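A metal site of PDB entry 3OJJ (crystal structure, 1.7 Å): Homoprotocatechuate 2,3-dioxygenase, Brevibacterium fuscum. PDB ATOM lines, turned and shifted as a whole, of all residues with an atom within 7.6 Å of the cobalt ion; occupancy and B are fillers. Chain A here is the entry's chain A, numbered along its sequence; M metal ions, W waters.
The side-chain carboxylate (OE2) of Glu 267 sits at hydrogen-bond distance from the side-chain hydroxyl (OH) of Tyr 257, at 3.3 Å.
A ring nitrogen (NE2) of His 248 sits at hydrogen-bond distance from the side-chain carboxylate of Glu 267 (2.8 Å).
The backbone carbonyl oxygen of Val 215 is in hydrogen-bond range of the backbone NH of Glu 267 (2.9 Å).
A ring nitrogen (ND1) of His 155 sits close to a ring nitrogen (NE2) of His 200, 3.3 Å away.
The backbone carbonyl oxygen (O) of His 155 lies within hydrogen-bond range of the backbone NH (N) of Ala 216, 2.8 Å away.
A ring nitrogen (ND1) of His 155 is in hydrogen-bond range of the side-chain carboxylate (OD2) of Asp 154 (2.8 Å).
The backbone NH (N) of Asn 157 lies within hydrogen-bond range of the backbone carbonyl oxygen (O) of His 214 (3.0 Å).
A ring nitrogen (ND1) of His 214 is in hydrogen-bond range of a ring nitrogen (ND1) of His 213.
Water W2 lies within hydrogen-bond range of NE2 of His 200 and ND2 of Asn 157.
The cobalt ion is bound by water W2, the side-chain carboxylate (OE1) of Glu 267, a ring nitrogen (NE2) of His 155, water W1, a ring nitrogen (NE2) of His 214 and water W3.
His 200 touches the cobalt ion (NE2 to CO, 3.8 Å).
The nearest printed residue that does not touch the cobalt ion is Tyr 257 (4.2 Å).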
ATOM      1  N   ASP A 154      17.533 -17.698   9.472  1.00  0.00           N
ATOM      2  CA  ASP A 154      16.692 -17.134  10.536  1.00  0.00           C
ATOM      3  C   ASP A 154      16.927 -17.758  11.915  1.00  0.00           C
ATOM      4  O   ASP A 154      17.031 -17.017  12.894  1.00  0.00           O
ATOM      5  CB  ASP A 154      15.194 -17.254  10.234  1.00  0.00           C
ATOM      6  CG  ASP A 154      14.357 -16.452  11.223  1.00  0.00           C
ATOM      7  OD1 ASP A 154      14.395 -15.190  11.144  1.00  0.00           O
ATOM      8  OD2 ASP A 154      13.759 -17.087  12.130  1.00  0.00           O
ATOM      9  N   HIS A 155      16.952 -19.081  12.009  1.00  0.00           N
ATOM     10  CA  HIS A 155      17.071 -19.709  13.331  1.00  0.00           C
ATOM     11  C   HIS A 155      17.520 -21.136  13.298  1.00  0.00           C
ATOM     12  O   HIS A 155      17.494 -21.779  12.266  1.00  0.00           O
ATOM     13  CB  HIS A 155      15.728 -19.637  14.114  1.00  0.00           C
ATOM     14  CG  HIS A 155      14.591 -20.400  13.504  1.00  0.00           C
ATOM     15  ND1 HIS A 155      13.658 -19.795  12.679  1.00  0.00           N
ATOM     16  CD2 HIS A 155      14.189 -21.693  13.628  1.00  0.00           C
ATOM     17  CE1 HIS A 155      12.748 -20.687  12.316  1.00  0.00           C
ATOM     18  NE2 HIS A 155      13.023 -21.842  12.896  1.00  0.00           N
ATOM     19  N   PHE A 156      17.893 -21.626  14.487  1.00  0.00           N
ATOM     20  CA  PHE A 156      18.059 -23.031  14.747  1.00  0.00           C
ATOM     21  C   PHE A 156      16.906 -23.501  15.657  1.00  0.00           C
ATOM     22  O   PHE A 156      16.206 -22.669  16.246  1.00  0.00           O
ATOM     23  CB  PHE A 156      19.363 -23.275  15.515  1.00  0.00           C
ATOM     24  CG  PHE A 156      20.594 -22.631  14.910  1.00  0.00           C
ATOM     25  CD1 PHE A 156      20.968 -22.861  13.611  1.00  0.00           C
ATOM     26  CD2 PHE A 156      21.406 -21.832  15.706  1.00  0.00           C
ATOM     27  CE1 PHE A 156      22.098 -22.275  13.100  1.00  0.00           C
ATOM     28  CE2 PHE A 156      22.536 -21.232  15.196  1.00  0.00           C
ATOM     29  CZ  PHE A 156      22.882 -21.454  13.893  1.00  0.00           C
ATOM     30  N   ASN A 157      16.703 -24.803  15.747  1.00  0.00           N
ATOM     31  CA  ASN A 157      15.748 -25.378  16.715  1.00  0.00           C
ATOM     32  C   ASN A 157      16.329 -26.677  17.241  1.00  0.00           C
ATOM     33  O   ASN A 157      16.691 -27.585  16.477  1.00  0.00           O
ATOM     34  CB  ASN A 157      14.383 -25.582  16.080  1.00  0.00           C
ATOM     35  CG  ASN A 157      13.319 -26.002  17.081  1.00  0.00           C
ATOM     36  OD1 ASN A 157      13.452 -27.002  17.718  1.00  0.00           O
ATOM     37  ND2 ASN A 157      12.205 -25.223  17.154  1.00  0.00           N
ATOM     38  N   TRP A 192      10.698 -20.478  22.486  1.00  0.00           N
ATOM     39  CA  TRP A 192      11.351 -19.767  21.407  1.00  0.00           C
ATOM     40  C   TRP A 192      12.055 -18.572  22.021  1.00  0.00           C
ATOM     41  O   TRP A 192      11.460 -17.862  22.825  1.00  0.00           O
ATOM     42  CB  TRP A 192      10.305 -19.279  20.402  1.00  0.00           C
ATOM     43  CG  TRP A 192       9.749 -20.350  19.491  1.00  0.00           C
ATOM     44  CD1 TRP A 192       9.981 -20.477  18.144  1.00  0.00           C
ATOM     45  CD2 TRP A 192       8.835 -21.413  19.835  1.00  0.00           C
ATOM     46  NE1 TRP A 192       9.288 -21.550  17.638  1.00  0.00           N
ATOM     47  CE2 TRP A 192       8.567 -22.129  18.636  1.00  0.00           C
ATOM     48  CE3 TRP A 192       8.157 -21.772  21.010  1.00  0.00           C
ATOM     49  CZ2 TRP A 192       7.704 -23.225  18.590  1.00  0.00           C
ATOM     50  CZ3 TRP A 192       7.316 -22.849  20.978  1.00  0.00           C
ATOM     51  CH2 TRP A 192       7.075 -23.571  19.766  1.00  0.00           C
ATOM     52  N   HIS A 200      12.800 -15.664  16.985  1.00  0.00           N
ATOM     53  CA  HIS A 200      13.882 -16.422  17.579  1.00  0.00           C
ATOM     54  C   HIS A 200      15.177 -16.462  16.784  1.00  0.00           C
ATOM     55  O   HIS A 200      15.203 -16.202  15.576  1.00  0.00           O
ATOM     56  CB  HIS A 200      13.426 -17.857  17.937  1.00  0.00           C
ATOM     57  CG  HIS A 200      12.850 -18.680  16.818  1.00  0.00           C
ATOM     58  ND1 HIS A 200      11.965 -18.184  15.880  1.00  0.00           N
ATOM     59  CD2 HIS A 200      12.913 -20.017  16.607  1.00  0.00           C
ATOM     60  CE1 HIS A 200      11.573 -19.182  15.098  1.00  0.00           C
ATOM     61  NE2 HIS A 200      12.111 -20.305  15.530  1.00  0.00           N
ATOM     62  N   ALA A 203      15.584 -22.168  19.474  1.00  0.00           N
ATOM     63  CA  ALA A 203      14.355 -22.610  20.115  1.00  0.00           C
ATOM     64  C   ALA A 203      14.579 -23.995  20.674  1.00  0.00           C
ATOM     65  O   ALA A 203      15.481 -24.723  20.234  1.00  0.00           O
ATOM     66  CB  ALA A 203      13.174 -22.603  19.106  1.00  0.00           C
ATOM     67  N   THR A 205      12.702 -27.573  21.644  1.00  0.00           N
ATOM     68  CA  THR A 205      11.595 -28.503  21.467  1.00  0.00           C
ATOM     69  C   THR A 205      11.850 -29.694  22.403  1.00  0.00           C
ATOM     70  O   THR A 205      12.940 -30.314  22.379  1.00  0.00           O
ATOM     71  CB  THR A 205      11.489 -29.008  20.017  1.00  0.00           C
ATOM     72  OG1 THR A 205      11.299 -27.896  19.127  1.00  0.00           O
ATOM     73  CG2 THR A 205      10.352 -30.034  19.875  1.00  0.00           C
ATOM     74  N   HIS A 213      16.757 -30.230  15.773  1.00  0.00           N
ATOM     75  CA  HIS A 213      15.507 -30.390  15.094  1.00  0.00           C
ATOM     76  C   HIS A 213      15.554 -29.838  13.654  1.00  0.00           C
ATOM     77  O   HIS A 213      15.198 -30.546  12.708  1.00  0.00           O
ATOM     78  CB  HIS A 213      14.350 -29.725  15.875  1.00  0.00           C
ATOM     79  CG  HIS A 213      13.027 -30.247  15.439  1.00  0.00           C
ATOM     80  ND1 HIS A 213      12.401 -29.811  14.290  1.00  0.00           N
ATOM     81  CD2 HIS A 213      12.250 -31.248  15.938  1.00  0.00           C
ATOM     82  CE1 HIS A 213      11.285 -30.486  14.121  1.00  0.00           C
ATOM     83  NE2 HIS A 213      11.168 -31.365  15.104  1.00  0.00           N
ATOM     84  N   HIS A 214      15.946 -28.567  13.481  1.00  0.00           N
ATOM     85  CA  HIS A 214      16.090 -28.008  12.138  1.00  0.00           C
ATOM     86  C   HIS A 214      16.910 -26.738  12.107  1.00  0.00           C
ATOM     87  O   HIS A 214      17.221 -26.133  13.152  1.00  0.00           O
ATOM     88  CB  HIS A 214      14.725 -27.748  11.490  1.00  0.00           C
ATOM     89  CG  HIS A 214      13.828 -26.834  12.273  1.00  0.00           C
ATOM     90  ND1 HIS A 214      12.911 -27.311  13.183  1.00  0.00           N
ATOM     91  CD2 HIS A 214      13.653 -25.494  12.249  1.00  0.00           C
ATOM     92  CE1 HIS A 214      12.243 -26.308  13.710  1.00  0.00           C
ATOM     93  NE2 HIS A 214      12.679 -25.178  13.164  1.00  0.00           N
ATOM     94  N   VAL A 215      17.294 -26.365  10.888  1.00  0.00           N
ATOM     95  CA  VAL A 215      17.831 -25.055  10.595  1.00  0.00           C
ATOM     96  C   VAL A 215      16.814 -24.347   9.697  1.00  0.00           C
ATOM     97  O   VAL A 215      16.239 -24.981   8.782  1.00  0.00           O
ATOM     98  CB  VAL A 215      19.210 -25.164   9.824  1.00  0.00           C
ATOM     99  CG1 VAL A 215      19.763 -23.807   9.489  1.00  0.00           C
ATOM    100  CG2 VAL A 215      20.215 -25.949  10.649  1.00  0.00           C
ATOM    101  N   ALA A 216      16.587 -23.049   9.919  1.00  0.00           N
ATOM    102  CA  ALA A 216      15.565 -22.313   9.153  1.00  0.00           C
ATOM    103  C   ALA A 216      16.162 -21.176   8.336  1.00  0.00           C
ATOM    104  O   ALA A 216      16.951 -20.387   8.864  1.00  0.00           O
ATOM    105  CB  ALA A 216      14.467 -21.757  10.106  1.00  0.00           C
ATOM    106  N   HIS A 248       2.207 -20.741  10.845  1.00  0.00           N
ATOM    107  CA  HIS A 248       2.412 -21.116  12.238  1.00  0.00           C
ATOM    108  C   HIS A 248       1.441 -20.342  13.128  1.00  0.00           C
ATOM    109  O   HIS A 248       1.067 -19.191  12.834  1.00  0.00           O
ATOM    110  CB  HIS A 248       3.841 -20.809  12.716  1.00  0.00           C
ATOM    111  CG  HIS A 248       4.875 -21.812  12.280  1.00  0.00           C
ATOM    112  ND1 HIS A 248       4.770 -23.160  12.547  1.00  0.00           N
ATOM    113  CD2 HIS A 248       6.074 -21.644  11.675  1.00  0.00           C
ATOM    114  CE1 HIS A 248       5.841 -23.784  12.093  1.00  0.00           C
ATOM    115  NE2 HIS A 248       6.651 -22.885  11.545  1.00  0.00           N
ATOM    116  N   SER A 251       4.815 -17.839  16.473  1.00  0.00           N
ATOM    117  CA  SER A 251       5.690 -17.060  15.549  1.00  0.00           C
ATOM    118  C   SER A 251       4.920 -16.374  14.428  1.00  0.00           C
ATOM    119  O   SER A 251       5.427 -15.444  13.810  1.00  0.00           O
ATOM    120  CB  SER A 251       6.836 -17.855  14.962  1.00  0.00           C
ATOM    121  OG  SER A 251       6.441 -18.626  13.840  1.00  0.00           O
ATOM    122  N   TYR A 255       5.431 -21.111   6.634  1.00  0.00           N
ATOM    123  CA  TYR A 255       6.492 -22.125   6.807  1.00  0.00           C
ATOM    124  C   TYR A 255       6.357 -23.338   5.917  1.00  0.00           C
ATOM    125  O   TYR A 255       5.294 -23.600   5.332  1.00  0.00           O
ATOM    126  CB  TYR A 255       6.532 -22.618   8.270  1.00  0.00           C
ATOM    127  CG  TYR A 255       5.398 -23.539   8.612  1.00  0.00           C
ATOM    128  CD1 TYR A 255       4.248 -23.065   9.202  1.00  0.00           C
ATOM    129  CD2 TYR A 255       5.508 -24.920   8.394  1.00  0.00           C
ATOM    130  CE1 TYR A 255       3.197 -23.902   9.529  1.00  0.00           C
ATOM    131  CE2 TYR A 255       4.465 -25.770   8.714  1.00  0.00           C
ATOM    132  CZ  TYR A 255       3.303 -25.270   9.272  1.00  0.00           C
ATOM    133  OH  TYR A 255       2.276 -26.123   9.615  1.00  0.00           O
ATOM    134  N   TYR A 257       8.602 -27.433   5.954  1.00  0.00           N
ATOM    135  CA  TYR A 257       9.705 -28.322   6.380  1.00  0.00           C
ATOM    136  C   TYR A 257       9.979 -29.366   5.298  1.00  0.00           C
ATOM    137  O   TYR A 257       9.075 -30.067   4.824  1.00  0.00           O
ATOM    138  CB  TYR A 257       9.338 -29.075   7.674  1.00  0.00           C
ATOM    139  CG  TYR A 257       9.068 -28.160   8.834  1.00  0.00           C
ATOM    140  CD1 TYR A 257      10.100 -27.647   9.584  1.00  0.00           C
ATOM    141  CD2 TYR A 257       7.766 -27.799   9.156  1.00  0.00           C
ATOM    142  CE1 TYR A 257       9.863 -26.787  10.649  1.00  0.00           C
ATOM    143  CE2 TYR A 257       7.503 -26.950  10.203  1.00  0.00           C
ATOM    144  CZ  TYR A 257       8.551 -26.452  10.957  1.00  0.00           C
ATOM    145  OH  TYR A 257       8.272 -25.632  12.011  1.00  0.00           O
ATOM    146  N   GLU A 267      13.798 -25.811   7.564  1.00  0.00           N
ATOM    147  CA  GLU A 267      12.546 -25.049   7.516  1.00  0.00           C
ATOM    148  C   GLU A 267      12.754 -23.853   6.599  1.00  0.00           C
ATOM    149  O   GLU A 267      13.801 -23.204   6.638  1.00  0.00           O
ATOM    150  CB  GLU A 267      12.148 -24.529   8.892  1.00  0.00           C
ATOM    151  CG  GLU A 267      10.737 -23.971   8.915  1.00  0.00           C
ATOM    152  CD  GLU A 267      10.377 -23.400  10.278  1.00  0.00           C
ATOM    153  OE1 GLU A 267      11.246 -23.516  11.141  1.00  0.00           O
ATOM    154  OE2 GLU A 267       9.253 -22.854  10.504  1.00  0.00           O
ATOM    155  N   ILE A 268      11.725 -23.551   5.821  1.00  0.00           N
ATOM    156  CA  ILE A 268      11.637 -22.296   5.080  1.00  0.00           C
ATOM    157  C   ILE A 268      10.556 -21.469   5.793  1.00  0.00           C
ATOM    158  O   ILE A 268       9.510 -21.989   6.153  1.00  0.00           O
ATOM    159  CB  ILE A 268      11.329 -22.495   3.567  1.00  0.00           C
ATOM    160  CG1 ILE A 268      12.030 -23.736   2.999  1.00  0.00           C
ATOM    161  CG2 ILE A 268      11.685 -21.212   2.774  1.00  0.00           C
ATOM    162  CD1 ILE A 268      13.481 -23.634   2.933  1.00  0.00           C
ATOM    163  N   TYR A 269      10.832 -20.195   6.036  1.00  0.00           N
ATOM    164  CA  TYR A 269      10.100 -19.408   6.997  1.00  0.00           C
ATOM    165  C   TYR A 269       9.969 -17.961   6.503  1.00  0.00           C
ATOM    166  O   TYR A 269      10.900 -17.404   5.922  1.00  0.00           O
ATOM    167  CB  TYR A 269      10.935 -19.466   8.275  1.00  0.00           C
ATOM    168  CG  TYR A 269      10.526 -18.767   9.534  1.00  0.00           C
ATOM    169  CD1 TYR A 269       9.815 -19.439  10.537  1.00  0.00           C
ATOM    170  CD2 TYR A 269      10.991 -17.477   9.833  1.00  0.00           C
ATOM    171  CE1 TYR A 269       9.513 -18.829  11.747  1.00  0.00           C
ATOM    172  CE2 TYR A 269      10.669 -16.842  11.017  1.00  0.00           C
ATOM    173  CZ  TYR A 269       9.945 -17.547  11.999  1.00  0.00           C
ATOM    174  OH  TYR A 269       9.663 -16.944  13.202  1.00  0.00           O
ATOM    175  N   ARG A 293       0.600 -24.845  16.300  1.00  0.00           N
ATOM    176  CA  ARG A 293       1.735 -25.180  15.449  1.00  0.00           C
ATOM    177  C   ARG A 293       1.408 -24.857  13.989  1.00  0.00           C
ATOM    178  O   ARG A 293       2.173 -24.176  13.311  1.00  0.00           O
ATOM    179  CB  ARG A 293       2.181 -26.637  15.663  1.00  0.00           C
ATOM    180  CG  ARG A 293       2.980 -26.807  16.934  1.00  0.00           C
ATOM    181  CD  ARG A 293       3.910 -28.013  16.963  1.00  0.00           C
ATOM    182  NE  ARG A 293       4.646 -28.095  18.223  1.00  0.00           N
ATOM    183  CZ  ARG A 293       5.796 -27.459  18.468  1.00  0.00           C
ATOM    184  NH1 ARG A 293       6.353 -26.660  17.571  1.00  0.00           N
ATOM    185  NH2 ARG A 293       6.372 -27.612  19.641  1.00  0.00           N
ATOM    186  N   TRP A 304       7.642 -35.387  12.622  1.00  0.00           N
ATOM    187  CA  TRP A 304       8.114 -34.071  13.000  1.00  0.00           C
ATOM    188  C   TRP A 304       8.462 -34.020  14.488  1.00  0.00           C
ATOM    189  O   TRP A 304       9.365 -33.311  14.893  1.00  0.00           O
ATOM    190  CB  TRP A 304       7.045 -33.015  12.652  1.00  0.00           C
ATOM    191  CG  TRP A 304       7.583 -31.626  12.654  1.00  0.00           C
ATOM    192  CD1 TRP A 304       8.130 -30.957  11.595  1.00  0.00           C
ATOM    193  CD2 TRP A 304       7.662 -30.730  13.762  1.00  0.00           C
ATOM    194  NE1 TRP A 304       8.506 -29.717  11.972  1.00  0.00           N
ATOM    195  CE2 TRP A 304       8.237 -29.551  13.307  1.00  0.00           C
ATOM    196  CE3 TRP A 304       7.301 -30.840  15.101  1.00  0.00           C
ATOM    197  CZ2 TRP A 304       8.461 -28.469  14.138  1.00  0.00           C
ATOM    198  CZ3 TRP A 304       7.516 -29.773  15.937  1.00  0.00           C
ATOM    199  CH2 TRP A 304       8.093 -28.611  15.450  1.00  0.00           C
HETATM  200 CO    CO M   1      11.519 -23.317  13.248  1.00  0.00          CO
HETATM  201  O   HOH W   1       9.902 -21.868  13.083  1.00  0.00           O
HETATM  202  O   HOH W   2      11.678 -22.978  15.346  1.00  0.00           O
HETATM  203  O   HOH W   3       9.709 -24.587  13.859  1.00  0.00           O
